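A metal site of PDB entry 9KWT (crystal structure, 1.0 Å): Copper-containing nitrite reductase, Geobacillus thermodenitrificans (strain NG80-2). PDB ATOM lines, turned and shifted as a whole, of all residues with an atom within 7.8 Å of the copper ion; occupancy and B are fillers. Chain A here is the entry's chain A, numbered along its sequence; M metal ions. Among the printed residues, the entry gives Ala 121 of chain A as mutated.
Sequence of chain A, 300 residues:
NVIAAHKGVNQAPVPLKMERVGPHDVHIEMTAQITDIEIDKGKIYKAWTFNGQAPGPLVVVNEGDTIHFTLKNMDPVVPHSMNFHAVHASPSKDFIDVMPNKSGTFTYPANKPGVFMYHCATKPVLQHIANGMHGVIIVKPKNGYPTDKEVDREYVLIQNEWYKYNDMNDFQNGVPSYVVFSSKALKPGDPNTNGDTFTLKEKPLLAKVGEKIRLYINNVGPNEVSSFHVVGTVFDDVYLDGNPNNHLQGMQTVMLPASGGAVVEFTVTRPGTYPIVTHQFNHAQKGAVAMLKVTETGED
The copper ion is bound by a ring nitrogen (ND1) of His 80 (2.0 Å).
The copper ion is bound by ND1 of His 128.
The copper ion is bound by the side-chain sulfur (SG) of Cys 120 (2.2 Å).
The copper ion is bound by SD of Met 133, at 2.6 Å.
The backbone carbonyl oxygen of Val 78 sits close to a ring nitrogen (NE2) of His 80 (3.4 Å).
OD2 of Asp 75 lies within hydrogen-bond range of NE2 of His 80, 2.8 Å away.
The side-chain amide nitrogen (ND2) of Asn 73 sits close to the backbone NH (N) of His 80 (3.5 Å).
SG of Cys 120 lies close to OG1 of Thr 122, 3.4 Å away.
The backbone NH (N) of Ser 81 sits close to the side-chain sulfur (SG) of Cys 120 (3.5 Å).
The backbone NH (N) of Met 133 lies close to the backbone carbonyl oxygen (O) of Trp 48, at 3.3 Å.
Four residues have an atom within 4 Å of the copper ion: His 80, Cys 120, His 128 and Met 133.
The nearest printed residue that does not touch the copper ion is Pro 79 (4.03 Å).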
ATOM      1  N   ALA A  32     -17.697 -18.885  -1.501  1.00  0.00           N
ATOM      2  CA  ALA A  32     -18.775 -18.043  -0.982  1.00  0.00           C
ATOM      3  C   ALA A  32     -18.112 -17.053  -0.030  1.00  0.00           C
ATOM      4  O   ALA A  32     -17.360 -17.467   0.860  1.00  0.00           O
ATOM      5  CB  ALA A  32     -19.839 -18.850  -0.250  1.00  0.00           C
ATOM      6  N   TRP A  48     -23.509 -10.887  -0.219  1.00  0.00           N
ATOM      7  CA  TRP A  48     -23.206 -12.303  -0.161  1.00  0.00           C
ATOM      8  C   TRP A  48     -22.901 -12.723  -1.592  1.00  0.00           C
ATOM      9  O   TRP A  48     -23.734 -12.501  -2.489  1.00  0.00           O
ATOM     10  CB  TRP A  48     -24.400 -13.080   0.380  1.00  0.00           C
ATOM     11  CG  TRP A  48     -24.871 -12.718   1.758  1.00  0.00           C
ATOM     12  CD1 TRP A  48     -24.490 -11.678   2.565  1.00  0.00           C
ATOM     13  CD2 TRP A  48     -25.867 -13.446   2.485  1.00  0.00           C
ATOM     14  NE1 TRP A  48     -25.189 -11.724   3.750  1.00  0.00           N
ATOM     15  CE2 TRP A  48     -26.042 -12.803   3.727  1.00  0.00           C
ATOM     16  CE3 TRP A  48     -26.656 -14.560   2.192  1.00  0.00           C
ATOM     17  CZ2 TRP A  48     -26.959 -13.249   4.668  1.00  0.00           C
ATOM     18  CZ3 TRP A  48     -27.568 -14.988   3.121  1.00  0.00           C
ATOM     19  CH2 TRP A  48     -27.713 -14.346   4.358  1.00  0.00           C
ATOM     20  N   THR A  49     -21.727 -13.305  -1.818  1.00  0.00           N
ATOM     21  CA  THR A  49     -21.228 -13.465  -3.181  1.00  0.00           C
ATOM     22  C   THR A  49     -20.580 -14.819  -3.395  1.00  0.00           C
ATOM     23  O   THR A  49     -20.128 -15.478  -2.454  1.00  0.00           O
ATOM     24  CB  THR A  49     -20.179 -12.407  -3.559  1.00  0.00           C
ATOM     25  OG1 THR A  49     -18.924 -12.713  -2.932  1.00  0.00           O
ATOM     26  CG2 THR A  49     -20.624 -11.009  -3.191  1.00  0.00           C
ATOM     27  N   PHE A  50     -20.472 -15.162  -4.668  1.00  0.00           N
ATOM     28  CA  PHE A  50     -19.465 -16.090  -5.142  1.00  0.00           C
ATOM     29  C   PHE A  50     -18.254 -15.283  -5.591  1.00  0.00           C
ATOM     30  O   PHE A  50     -18.361 -14.407  -6.469  1.00  0.00           O
ATOM     31  CB  PHE A  50     -20.009 -16.927  -6.297  1.00  0.00           C
ATOM     32  CG  PHE A  50     -21.170 -17.808  -5.899  1.00  0.00           C
ATOM     33  CD1 PHE A  50     -20.969 -18.932  -5.130  1.00  0.00           C
ATOM     34  CD2 PHE A  50     -22.464 -17.475  -6.284  1.00  0.00           C
ATOM     35  CE1 PHE A  50     -22.044 -19.737  -4.768  1.00  0.00           C
ATOM     36  CE2 PHE A  50     -23.532 -18.285  -5.917  1.00  0.00           C
ATOM     37  CZ  PHE A  50     -23.313 -19.423  -5.171  1.00  0.00           C
ATOM     38  N   LEU A  71     -17.114 -25.749  -3.754  1.00  0.00           N
ATOM     39  CA  LEU A  71     -17.410 -24.480  -3.090  1.00  0.00           C
ATOM     40  C   LEU A  71     -16.644 -24.419  -1.786  1.00  0.00           C
ATOM     41  O   LEU A  71     -16.791 -25.300  -0.938  1.00  0.00           O
ATOM     42  CB  LEU A  71     -18.906 -24.357  -2.807  1.00  0.00           C
ATOM     43  CG  LEU A  71     -19.349 -23.021  -2.203  1.00  0.00           C
ATOM     44  CD1 LEU A  71     -19.114 -21.870  -3.169  1.00  0.00           C
ATOM     45  CD2 LEU A  71     -20.814 -23.093  -1.808  1.00  0.00           C
ATOM     46  N   ASN A  73     -16.492 -22.244   1.433  1.00  0.00           N
ATOM     47  CA  ASN A  73     -17.310 -21.269   2.128  1.00  0.00           C
ATOM     48  C   ASN A  73     -16.447 -20.439   3.089  1.00  0.00           C
ATOM     49  O   ASN A  73     -16.009 -20.950   4.122  1.00  0.00           O
ATOM     50  CB  ASN A  73     -18.475 -21.916   2.867  1.00  0.00           C
ATOM     51  CG  ASN A  73     -19.431 -20.889   3.429  1.00  0.00           C
ATOM     52  OD1 ASN A  73     -19.236 -19.688   3.252  1.00  0.00           O
ATOM     53  ND2 ASN A  73     -20.447 -21.357   4.136  1.00  0.00           N
ATOM     54  N   ASP A  75     -17.645 -17.530   4.375  1.00  0.00           N
ATOM     55  CA  ASP A  75     -18.525 -16.805   5.277  1.00  0.00           C
ATOM     56  C   ASP A  75     -18.305 -17.327   6.693  1.00  0.00           C
ATOM     57  O   ASP A  75     -18.314 -18.549   6.893  1.00  0.00           O
ATOM     58  CB  ASP A  75     -19.971 -17.051   4.829  1.00  0.00           C
ATOM     59  CG  ASP A  75     -21.017 -16.207   5.560  1.00  0.00           C
ATOM     60  OD1 ASP A  75     -20.906 -16.031   6.803  1.00  0.00           O
ATOM     61  OD2 ASP A  75     -21.981 -15.755   4.899  1.00  0.00           O
ATOM     62  N   VAL A  78     -22.685 -18.113   7.948  1.00  0.00           N
ATOM     63  CA  VAL A  78     -23.821 -18.569   7.149  1.00  0.00           C
ATOM     64  C   VAL A  78     -23.391 -19.700   6.221  1.00  0.00           C
ATOM     65  O   VAL A  78     -22.410 -19.539   5.484  1.00  0.00           O
ATOM     66  CB  VAL A  78     -24.479 -17.433   6.350  1.00  0.00           C
ATOM     67  CG1 VAL A  78     -25.785 -17.914   5.732  1.00  0.00           C
ATOM     68  CG2 VAL A  78     -24.722 -16.205   7.210  1.00  0.00           C
ATOM     69  N   PRO A  79     -24.101 -20.841   6.204  1.00  0.00           N
ATOM     70  CA  PRO A  79     -23.865 -21.851   5.172  1.00  0.00           C
ATOM     71  C   PRO A  79     -24.246 -21.322   3.783  1.00  0.00           C
ATOM     72  O   PRO A  79     -25.105 -20.454   3.653  1.00  0.00           O
ATOM     73  CB  PRO A  79     -24.789 -23.003   5.575  1.00  0.00           C
ATOM     74  CG  PRO A  79     -25.092 -22.765   7.030  1.00  0.00           C
ATOM     75  CD  PRO A  79     -25.155 -21.277   7.138  1.00  0.00           C
ATOM     76  N   HIS A  80     -23.613 -21.888   2.754  1.00  0.00           N
ATOM     77  CA  HIS A  80     -23.930 -21.565   1.370  1.00  0.00           C
ATOM     78  C   HIS A  80     -23.863 -22.823   0.523  1.00  0.00           C
ATOM     79  O   HIS A  80     -23.364 -23.861   0.946  1.00  0.00           O
ATOM     80  CB  HIS A  80     -23.005 -20.476   0.814  1.00  0.00           C
ATOM     81  CG  HIS A  80     -23.132 -19.185   1.554  1.00  0.00           C
ATOM     82  ND1 HIS A  80     -24.251 -18.376   1.454  1.00  0.00           N
ATOM     83  CD2 HIS A  80     -22.303 -18.591   2.449  1.00  0.00           C
ATOM     84  CE1 HIS A  80     -24.083 -17.330   2.242  1.00  0.00           C
ATOM     85  NE2 HIS A  80     -22.919 -17.446   2.871  1.00  0.00           N
ATOM     86  N   SER A  81     -24.357 -22.713  -0.713  1.00  0.00           N
ATOM     87  CA  SER A  81     -24.481 -23.862  -1.594  1.00  0.00           C
ATOM     88  C   SER A  81     -24.503 -23.353  -3.039  1.00  0.00           C
ATOM     89  O   SER A  81     -24.431 -22.146  -3.292  1.00  0.00           O
ATOM     90  CB  SER A  81     -25.769 -24.632  -1.307  1.00  0.00           C
ATOM     91  OG  SER A  81     -26.901 -23.772  -1.420  1.00  0.00           O
ATOM     92  N   MET A  82     -24.622 -24.285  -3.981  1.00  0.00           N
ATOM     93  CA  MET A  82     -24.638 -23.945  -5.396  1.00  0.00           C
ATOM     94  C   MET A  82     -25.645 -24.797  -6.149  1.00  0.00           C
ATOM     95  O   MET A  82     -25.636 -26.027  -6.049  1.00  0.00           O
ATOM     96  CB  MET A  82     -23.257 -24.161  -6.027  1.00  0.00           C
ATOM     97  CG  MET A  82     -23.213 -23.986  -7.539  1.00  0.00           C
ATOM     98  SD  MET A  82     -23.644 -22.308  -8.090  1.00  0.00           S
ATOM     99  CE  MET A  82     -22.036 -21.518  -7.895  1.00  0.00           C
ATOM    100  N   ASP A  97     -25.717 -27.746   1.485  1.00  0.00           N
ATOM    101  CA  ASP A  97     -24.957 -26.705   2.139  1.00  0.00           C
ATOM    102  C   ASP A  97     -23.520 -27.122   2.423  1.00  0.00           C
ATOM    103  O   ASP A  97     -23.210 -28.278   2.721  1.00  0.00           O
ATOM    104  CB  ASP A  97     -25.625 -26.328   3.460  1.00  0.00           C
ATOM    105  CG  ASP A  97     -26.904 -25.546   3.264  1.00  0.00           C
ATOM    106  OD1 ASP A  97     -27.167 -25.057   2.143  1.00  0.00           O
ATOM    107  OD2 ASP A  97     -27.684 -25.444   4.237  1.00  0.00           O
ATOM    108  N   HIS A 119     -26.968 -20.064  -8.810  1.00  0.00           N
ATOM    109  CA  HIS A 119     -27.228 -19.298  -7.605  1.00  0.00           C
ATOM    110  C   HIS A 119     -27.065 -20.182  -6.370  1.00  0.00           C
ATOM    111  O   HIS A 119     -27.113 -21.406  -6.456  1.00  0.00           O
ATOM    112  CB  HIS A 119     -28.655 -18.702  -7.630  1.00  0.00           C
ATOM    113  CG  HIS A 119     -29.735 -19.723  -7.769  1.00  0.00           C
ATOM    114  ND1 HIS A 119     -30.282 -20.388  -6.700  1.00  0.00           N
ATOM    115  CD2 HIS A 119     -30.401 -20.175  -8.865  1.00  0.00           C
ATOM    116  CE1 HIS A 119     -31.244 -21.197  -7.132  1.00  0.00           C
ATOM    117  NE2 HIS A 119     -31.322 -21.099  -8.443  1.00  0.00           N
ATOM    118  N   CYS A 120     -26.939 -19.537  -5.222  1.00  0.00           N
ATOM    119  CA  CYS A 120     -26.955 -20.270  -3.974  1.00  0.00           C
ATOM    120  C   CYS A 120     -28.348 -20.867  -3.749  1.00  0.00           C
ATOM    121  O   CYS A 120     -29.365 -20.268  -4.103  1.00  0.00           O
ATOM    122  CB  CYS A 120     -26.546 -19.330  -2.840  1.00  0.00           C
ATOM    123  SG  CYS A 120     -26.561 -20.097  -1.215  1.00  0.00           S
ATOM    124  N   ALA A 121     -28.360 -22.059  -3.142  1.00  0.00           N
ATOM    125  CA  ALA A 121     -29.549 -22.866  -2.946  1.00  0.00           C
ATOM    126  C   ALA A 121     -29.916 -23.015  -1.472  1.00  0.00           C
ATOM    127  O   ALA A 121     -30.728 -23.883  -1.143  1.00  0.00           O
ATOM    128  CB  ALA A 121     -29.361 -24.255  -3.585  1.00  0.00           C
ATOM    129  N   THR A 122     -29.321 -22.227  -0.580  1.00  0.00           N
ATOM    130  CA  THR A 122     -29.531 -22.389   0.845  1.00  0.00           C
ATOM    131  C   THR A 122     -30.794 -21.658   1.284  1.00  0.00           C
ATOM    132  O   THR A 122     -31.068 -20.537   0.869  1.00  0.00           O
ATOM    133  CB  THR A 122     -28.302 -21.826   1.565  1.00  0.00           C
ATOM    134  OG1 THR A 122     -27.134 -22.552   1.130  1.00  0.00           O
ATOM    135  CG2 THR A 122     -28.425 -21.895   3.077  1.00  0.00           C
ATOM    136  N   LYS A 123     -31.582 -22.313   2.145  1.00  0.00           N
ATOM    137  CA  LYS A 123     -32.827 -21.732   2.615  1.00  0.00           C
ATOM    138  C   LYS A 123     -32.532 -20.584   3.589  1.00  0.00           C
ATOM    139  O   LYS A 123     -31.667 -20.714   4.466  1.00  0.00           O
ATOM    140  CB  LYS A 123     -33.668 -22.795   3.327  1.00  0.00           C
ATOM    141  CG  LYS A 123     -34.943 -22.278   3.993  1.00  0.00           C
ATOM    142  CD  LYS A 123     -36.016 -23.378   4.127  1.00  0.00           C
ATOM    143  CE  LYS A 123     -37.218 -22.906   4.934  1.00  0.00           C
ATOM    144  NZ  LYS A 123     -37.272 -23.488   6.293  1.00  0.00           N
ATOM    145  N   PRO A 124     -33.251 -19.452   3.489  1.00  0.00           N
ATOM    146  CA  PRO A 124     -34.239 -19.104   2.454  1.00  0.00           C
ATOM    147  C   PRO A 124     -33.546 -18.690   1.166  1.00  0.00           C
ATOM    148  O   PRO A 124     -32.696 -17.781   1.169  1.00  0.00           O
ATOM    149  CB  PRO A 124     -34.999 -17.910   3.049  1.00  0.00           C
ATOM    150  CG  PRO A 124     -34.478 -17.720   4.405  1.00  0.00           C
ATOM    151  CD  PRO A 124     -33.168 -18.409   4.520  1.00  0.00           C
ATOM    152  N   VAL A 125     -33.888 -19.354   0.064  1.00  0.00           N
ATOM    153  CA  VAL A 125     -33.199 -19.093  -1.183  1.00  0.00           C
ATOM    154  C   VAL A 125     -33.355 -17.629  -1.600  1.00  0.00           C
ATOM    155  O   VAL A 125     -32.406 -17.015  -2.112  1.00  0.00           O
ATOM    156  CB  VAL A 125     -33.664 -20.077  -2.273  1.00  0.00           C
ATOM    157  CG1 VAL A 125     -33.054 -19.744  -3.620  1.00  0.00           C
ATOM    158  CG2 VAL A 125     -33.303 -21.507  -1.866  1.00  0.00           C
ATOM    159  N   GLN A 127     -33.358 -15.057   0.226  1.00  0.00           N
ATOM    160  CA  GLN A 127     -32.379 -14.249   0.954  1.00  0.00           C
ATOM    161  C   GLN A 127     -30.991 -14.354   0.323  1.00  0.00           C
ATOM    162  O   GLN A 127     -30.290 -13.352   0.163  1.00  0.00           O
ATOM    163  CB  GLN A 127     -32.345 -14.699   2.422  1.00  0.00           C
ATOM    164  CG  GLN A 127     -31.464 -13.842   3.295  1.00  0.00           C
ATOM    165  CD  GLN A 127     -31.541 -14.219   4.755  1.00  0.00           C
ATOM    166  OE1 GLN A 127     -31.996 -15.305   5.101  1.00  0.00           O
ATOM    167  NE2 GLN A 127     -31.102 -13.312   5.612  1.00  0.00           N
ATOM    168  N   HIS A 128     -30.573 -15.575  -0.010  1.00  0.00           N
ATOM    169  CA  HIS A 128     -29.251 -15.771  -0.567  1.00  0.00           C
ATOM    170  C   HIS A 128     -29.134 -15.162  -1.957  1.00  0.00           C
ATOM    171  O   HIS A 128     -28.118 -14.529  -2.275  1.00  0.00           O
ATOM    172  CB  HIS A 128     -28.886 -17.248  -0.542  1.00  0.00           C
ATOM    173  CG  HIS A 128     -28.621 -17.764   0.829  1.00  0.00           C
ATOM    174  ND1 HIS A 128     -27.341 -18.036   1.279  1.00  0.00           N
ATOM    175  CD2 HIS A 128     -29.447 -17.994   1.872  1.00  0.00           C
ATOM    176  CE1 HIS A 128     -27.407 -18.456   2.526  1.00  0.00           C
ATOM    177  NE2 HIS A 128     -28.677 -18.425   2.911  1.00  0.00           N
ATOM    178  N   ILE A 129     -30.160 -15.334  -2.806  1.00  0.00           N
ATOM    179  CA  ILE A 129     -30.125 -14.696  -4.120  1.00  0.00           C
ATOM    180  C   ILE A 129     -30.152 -13.180  -3.976  1.00  0.00           C
ATOM    181  O   ILE A 129     -29.322 -12.476  -4.570  1.00  0.00           O
ATOM    182  CB  ILE A 129     -31.282 -15.195  -5.016  1.00  0.00           C
ATOM    183  CG1 ILE A 129     -31.184 -16.699  -5.264  1.00  0.00           C
ATOM    184  CG2 ILE A 129     -31.240 -14.439  -6.347  1.00  0.00           C
ATOM    185  CD1 ILE A 129     -32.328 -17.266  -6.124  1.00  0.00           C
ATOM    186  N   ASN A 131     -29.269 -11.191  -1.696  1.00  0.00           N
ATOM    187  CA  ASN A 131     -28.042 -10.603  -1.165  1.00  0.00           C
ATOM    188  C   ASN A 131     -26.858 -10.697  -2.108  1.00  0.00           C
ATOM    189  O   ASN A 131     -25.811 -10.108  -1.805  1.00  0.00           O
ATOM    190  CB  ASN A 131     -27.673 -11.232   0.180  1.00  0.00           C
ATOM    191  CG  ASN A 131     -28.488 -10.676   1.341  1.00  0.00           C
ATOM    192  OD1 ASN A 131     -28.846  -9.496   1.383  1.00  0.00           O
ATOM    193  ND2 ASN A 131     -28.744 -11.521   2.316  1.00  0.00           N
ATOM    194  N   GLY A 132     -26.994 -11.367  -3.266  1.00  0.00           N
ATOM    195  CA  GLY A 132     -25.994 -11.316  -4.303  1.00  0.00           C
ATOM    196  C   GLY A 132     -25.541 -12.634  -4.882  1.00  0.00           C
ATOM    197  O   GLY A 132     -24.703 -12.625  -5.786  1.00  0.00           O
ATOM    198  N   MET A 133     -26.065 -13.767  -4.407  1.00  0.00           N
ATOM    199  CA  MET A 133     -25.523 -15.075  -4.794  1.00  0.00           C
ATOM    200  C   MET A 133     -26.205 -15.632  -6.040  1.00  0.00           C
ATOM    201  O   MET A 133     -26.967 -16.594  -5.979  1.00  0.00           O
ATOM    202  CB  MET A 133     -25.525 -16.062  -3.641  1.00  0.00           C
ATOM    203  CG  MET A 133     -24.888 -15.493  -2.397  1.00  0.00           C
ATOM    204  SD  MET A 133     -24.513 -16.669  -1.074  1.00  0.00           S
ATOM    205  CE  MET A 133     -23.113 -17.494  -1.790  1.00  0.00           C
HETATM  206 CU    CU M   1     -25.759 -18.563   0.150  1.00  0.00          CU
